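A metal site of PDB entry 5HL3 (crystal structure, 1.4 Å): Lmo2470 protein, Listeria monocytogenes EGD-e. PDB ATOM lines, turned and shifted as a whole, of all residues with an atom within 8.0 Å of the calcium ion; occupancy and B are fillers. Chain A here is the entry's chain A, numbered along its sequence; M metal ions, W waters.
The backbone carbonyl oxygen (O) of Gly 267 sits at hydrogen-bond distance from the backbone NH (N) of Asp 355, at 3.0 Å.
The side-chain hydroxyl (OG) of Ser 341 lies close to the side-chain hydroxyl (OG) of Ser 353 (3.2 Å).
O of Ser 353 sits at hydrogen-bond distance from N of Gly 267 (3.2 Å).
The backbone carbonyl oxygen (O) of Gln 265 is in hydrogen-bond range of the backbone NH (N) of Ser 353, 2.9 Å away.
The side-chain hydroxyl (OG) of Ser 341 lies within hydrogen-bond range of the side-chain carboxylate (OD1) of Asp 339 (2.8 Å).
O of Asp 339 lies within hydrogen-bond range of N of Glu 304, at 3.0 Å.
Of the 16 residues printed, 3 come within 4 Å of the calcium ion.
The nearest printed residue that does not touch the calcium ion is Tyr 354 (4.6 Å).
The calcium ion is bound by water W4 (2.3 Å).
OD1 of Asp 355 binds the calcium ion, at 2.3 Å.
The side-chain hydroxyl (OG) of Ser 353 is bound to the calcium ion (2.4 Å).
The calcium ion is bound by water W3 (2.4 Å).
Water W1 is bound to the calcium ion (2.4 Å).
The calcium ion is bound by water W2, at 2.5 Å.
The calcium ion is bound by the side-chain carboxylate (OD2) of Asp 339 (2.5 Å).
Water W2 lies within hydrogen-bond range of the side-chain amide nitrogen (ND2) of Asn 266 (3.0 Å) and the backbone carbonyl oxygen (O) of Ser 353 (3.0 Å).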
ATOM      1  N   GLN A 265      -7.929 -15.205   1.912  1.00  0.00           N
ATOM      2  CA  GLN A 265      -6.788 -14.511   2.549  1.00  0.00           C
ATOM      3  C   GLN A 265      -5.850 -14.070   1.472  1.00  0.00           C
ATOM      4  O   GLN A 265      -5.788 -14.691   0.423  1.00  0.00           O
ATOM      5  CB  GLN A 265      -6.093 -15.484   3.532  1.00  0.00           C
ATOM      6  CG  GLN A 265      -5.266 -14.859   4.662  1.00  0.00           C
ATOM      7  CD  GLN A 265      -6.036 -14.278   5.853  1.00  0.00           C
ATOM      8  OE1 GLN A 265      -5.418 -13.706   6.748  1.00  0.00           O
ATOM      9  NE2 GLN A 265      -7.336 -14.451   5.891  1.00  0.00           N
ATOM     10  N   ASN A 266      -5.125 -13.016   1.724  1.00  0.00           N
ATOM     11  CA  ASN A 266      -4.123 -12.521   0.789  1.00  0.00           C
ATOM     12  C   ASN A 266      -2.821 -12.290   1.558  1.00  0.00           C
ATOM     13  O   ASN A 266      -2.772 -12.402   2.796  1.00  0.00           O
ATOM     14  CB  ASN A 266      -4.637 -11.273   0.085  1.00  0.00           C
ATOM     15  CG  ASN A 266      -5.838 -11.546  -0.775  1.00  0.00           C
ATOM     16  OD1 ASN A 266      -6.968 -11.623  -0.284  1.00  0.00           O
ATOM     17  ND2 ASN A 266      -5.614 -11.766  -2.049  1.00  0.00           N
ATOM     18  N   GLY A 267      -1.715 -12.167   0.855  1.00  0.00           N
ATOM     19  CA  GLY A 267      -0.500 -11.859   1.544  1.00  0.00           C
ATOM     20  C   GLY A 267       0.657 -11.608   0.623  1.00  0.00           C
ATOM     21  O   GLY A 267       0.548 -11.831  -0.590  1.00  0.00           O
ATOM     22  N   GLU A 268       1.736 -11.138   1.210  1.00  0.00           N
ATOM     23  CA  GLU A 268       2.974 -10.836   0.502  1.00  0.00           C
ATOM     24  C   GLU A 268       4.075 -11.681   1.121  1.00  0.00           C
ATOM     25  O   GLU A 268       4.204 -11.760   2.356  1.00  0.00           O
ATOM     26  CB  GLU A 268       3.343  -9.358   0.662  1.00  0.00           C
ATOM     27  CG  GLU A 268       2.300  -8.358   0.188  1.00  0.00           C
ATOM     28  CD  GLU A 268       2.035  -8.304  -1.325  1.00  0.00           C
ATOM     29  OE1 GLU A 268       2.996  -8.265  -2.145  1.00  0.00           O
ATOM     30  OE2 GLU A 268       0.856  -8.188  -1.690  1.00  0.00           O
ATOM     31  N   GLU A 304       1.481 -18.576 -10.953  1.00  0.00           N
ATOM     32  CA  GLU A 304       1.467 -17.796 -12.173  1.00  0.00           C
ATOM     33  C   GLU A 304       2.405 -16.614 -12.032  1.00  0.00           C
ATOM     34  O   GLU A 304       2.824 -16.290 -10.922  1.00  0.00           O
ATOM     35  CB  GLU A 304       0.054 -17.296 -12.469  1.00  0.00           C
ATOM     36  CG  GLU A 304      -0.471 -16.320 -11.428  1.00  0.00           C
ATOM     37  CD  GLU A 304      -1.951 -16.033 -11.545  1.00  0.00           C
ATOM     38  OE1 GLU A 304      -2.708 -16.866 -12.066  1.00  0.00           O
ATOM     39  OE2 GLU A 304      -2.386 -14.976 -11.048  1.00  0.00           O
ATOM     40  N   ILE A 306       2.795 -12.452 -13.519  1.00  0.00           N
ATOM     41  CA  ILE A 306       1.907 -11.379 -13.956  1.00  0.00           C
ATOM     42  C   ILE A 306       2.723 -10.339 -14.651  1.00  0.00           C
ATOM     43  O   ILE A 306       3.486  -9.632 -14.012  1.00  0.00           O
ATOM     44  CB  ILE A 306       1.177 -10.717 -12.746  1.00  0.00           C
ATOM     45  CG1 ILE A 306       0.384 -11.761 -11.908  1.00  0.00           C
ATOM     46  CG2 ILE A 306       0.319  -9.524 -13.174  1.00  0.00           C
ATOM     47  CD1 ILE A 306       1.123 -12.311 -10.692  1.00  0.00           C
ATOM     48  N   LEU A 338       5.194 -12.795  -8.967  1.00  0.00           N
ATOM     49  CA  LEU A 338       4.686 -14.183  -8.852  1.00  0.00           C
ATOM     50  C   LEU A 338       3.492 -14.234  -7.903  1.00  0.00           C
ATOM     51  O   LEU A 338       3.372 -13.413  -6.991  1.00  0.00           O
ATOM     52  CB  LEU A 338       5.780 -15.143  -8.348  1.00  0.00           C
ATOM     53  CG  LEU A 338       6.662 -15.791  -9.426  1.00  0.00           C
ATOM     54  CD1 LEU A 338       7.357 -14.775 -10.308  1.00  0.00           C
ATOM     55  CD2 LEU A 338       7.678 -16.774  -8.834  1.00  0.00           C
ATOM     56  N   ASP A 339       2.626 -15.210  -8.127  1.00  0.00           N
ATOM     57  CA  ASP A 339       1.438 -15.462  -7.313  1.00  0.00           C
ATOM     58  C   ASP A 339       1.238 -16.942  -7.152  1.00  0.00           C
ATOM     59  O   ASP A 339       1.366 -17.682  -8.130  1.00  0.00           O
ATOM     60  CB  ASP A 339       0.194 -14.862  -7.959  1.00  0.00           C
ATOM     61  CG  ASP A 339      -1.091 -15.366  -7.352  1.00  0.00           C
ATOM     62  OD1 ASP A 339      -1.425 -16.570  -7.412  1.00  0.00           O
ATOM     63  OD2 ASP A 339      -1.839 -14.538  -6.878  1.00  0.00           O
ATOM     64  N   VAL A 340       1.023 -17.396  -5.913  1.00  0.00           N
ATOM     65  CA  VAL A 340       0.549 -18.756  -5.641  1.00  0.00           C
ATOM     66  C   VAL A 340      -0.825 -18.619  -4.995  1.00  0.00           C
ATOM     67  O   VAL A 340      -1.008 -17.846  -4.031  1.00  0.00           O
ATOM     68  CB  VAL A 340       1.512 -19.540  -4.732  1.00  0.00           C
ATOM     69  CG1 VAL A 340       0.849 -20.774  -4.102  1.00  0.00           C
ATOM     70  CG2 VAL A 340       2.693 -20.013  -5.527  1.00  0.00           C
ATOM     71  N   SER A 341      -1.768 -19.366  -5.524  1.00  0.00           N
ATOM     72  CA  SER A 341      -3.149 -19.333  -5.050  1.00  0.00           C
ATOM     73  C   SER A 341      -3.648 -20.736  -4.742  1.00  0.00           C
ATOM     74  O   SER A 341      -3.258 -21.701  -5.414  1.00  0.00           O
ATOM     75  CB  SER A 341      -4.043 -18.651  -6.075  1.00  0.00           C
ATOM     76  OG  SER A 341      -3.777 -17.234  -6.127  1.00  0.00           O
ATOM     77  N   VAL A 351     -10.750 -17.172  -2.471  1.00  0.00           N
ATOM     78  CA  VAL A 351      -9.423 -17.662  -2.835  1.00  0.00           C
ATOM     79  C   VAL A 351      -8.428 -17.212  -1.767  1.00  0.00           C
ATOM     80  O   VAL A 351      -8.627 -16.197  -1.123  1.00  0.00           O
ATOM     81  CB  VAL A 351      -8.975 -17.170  -4.237  1.00  0.00           C
ATOM     82  CG1 VAL A 351      -8.773 -15.682  -4.259  1.00  0.00           C
ATOM     83  CG2 VAL A 351      -7.706 -17.880  -4.697  1.00  0.00           C
ATOM     84  N   CYS A 352      -7.365 -18.002  -1.592  1.00  0.00           N
ATOM     85  CA  CYS A 352      -6.208 -17.633  -0.799  1.00  0.00           C
ATOM     86  C   CYS A 352      -5.063 -17.379  -1.780  1.00  0.00           C
ATOM     87  O   CYS A 352      -4.702 -18.270  -2.524  1.00  0.00           O
ATOM     88  CB  CYS A 352      -5.853 -18.714   0.213  1.00  0.00           C
ATOM     89  SG  CYS A 352      -7.074 -18.903   1.555  1.00  0.00           S
ATOM     90  N   SER A 353      -4.530 -16.153  -1.803  1.00  0.00           N
ATOM     91  CA  SER A 353      -3.567 -15.761  -2.853  1.00  0.00           C
ATOM     92  C   SER A 353      -2.413 -14.965  -2.274  1.00  0.00           C
ATOM     93  O   SER A 353      -2.623 -14.026  -1.521  1.00  0.00           O
ATOM     94  CB  SER A 353      -4.292 -14.882  -3.879  1.00  0.00           C
ATOM     95  OG  SER A 353      -3.401 -14.330  -4.839  1.00  0.00           O
ATOM     96  N   TYR A 354      -1.195 -15.381  -2.612  1.00  0.00           N
ATOM     97  CA  TYR A 354       0.046 -14.829  -2.055  1.00  0.00           C
ATOM     98  C   TYR A 354       0.964 -14.402  -3.177  1.00  0.00           C
ATOM     99  O   TYR A 354       1.289 -15.205  -4.045  1.00  0.00           O
ATOM    100  CB  TYR A 354       0.706 -15.846  -1.119  1.00  0.00           C
ATOM    101  CG  TYR A 354      -0.164 -16.051   0.102  1.00  0.00           C
ATOM    102  CD1 TYR A 354      -1.230 -16.942   0.082  1.00  0.00           C
ATOM    103  CD2 TYR A 354      -0.001 -15.238   1.214  1.00  0.00           C
ATOM    104  CE1 TYR A 354      -2.080 -17.035   1.176  1.00  0.00           C
ATOM    105  CE2 TYR A 354      -0.827 -15.361   2.323  1.00  0.00           C
ATOM    106  CZ  TYR A 354      -1.881 -16.237   2.275  1.00  0.00           C
ATOM    107  OH  TYR A 354      -2.769 -16.318   3.351  1.00  0.00           O
ATOM    108  N   ASP A 355       1.468 -13.177  -3.080  1.00  0.00           N
ATOM    109  CA  ASP A 355       2.285 -12.567  -4.113  1.00  0.00           C
ATOM    110  C   ASP A 355       3.701 -12.334  -3.630  1.00  0.00           C
ATOM    111  O   ASP A 355       3.903 -12.062  -2.448  1.00  0.00           O
ATOM    112  CB  ASP A 355       1.722 -11.184  -4.441  1.00  0.00           C
ATOM    113  CG  ASP A 355       0.311 -11.202  -4.904  1.00  0.00           C
ATOM    114  OD1 ASP A 355      -0.258 -12.265  -5.197  1.00  0.00           O
ATOM    115  OD2 ASP A 355      -0.227 -10.093  -4.988  1.00  0.00           O
ATOM    116  N   TRP A 356       4.666 -12.309  -4.547  1.00  0.00           N
ATOM    117  CA  TRP A 356       6.032 -11.887  -4.203  1.00  0.00           C
ATOM    118  C   TRP A 356       6.757 -11.513  -5.468  1.00  0.00           C
ATOM    119  O   TRP A 356       6.360 -11.877  -6.561  1.00  0.00           O
ATOM    120  CB  TRP A 356       6.802 -12.949  -3.383  1.00  0.00           C
ATOM    121  CG  TRP A 356       7.251 -14.184  -4.140  1.00  0.00           C
ATOM    122  CD1 TRP A 356       8.529 -14.461  -4.538  1.00  0.00           C
ATOM    123  CD2 TRP A 356       6.462 -15.330  -4.519  1.00  0.00           C
ATOM    124  NE1 TRP A 356       8.590 -15.674  -5.160  1.00  0.00           N
ATOM    125  CE2 TRP A 356       7.328 -16.222  -5.166  1.00  0.00           C
ATOM    126  CE3 TRP A 356       5.129 -15.672  -4.397  1.00  0.00           C
ATOM    127  CZ2 TRP A 356       6.902 -17.427  -5.677  1.00  0.00           C
ATOM    128  CZ3 TRP A 356       4.708 -16.889  -4.919  1.00  0.00           C
ATOM    129  CH2 TRP A 356       5.590 -17.742  -5.565  1.00  0.00           C
HETATM  130 CA    CA M   1      -2.509 -12.355  -5.841  1.00  0.00          CA
HETATM  131  O   HOH W   1      -1.906 -11.602  -8.070  1.00  0.00           O
HETATM  132  O   HOH W   2      -3.001 -11.782  -3.473  1.00  0.00           O
HETATM  133  O   HOH W   3      -2.837  -9.971  -5.875  1.00  0.00           O
HETATM  134  O   HOH W   4      -4.647 -12.371  -6.691  1.00  0.00           O
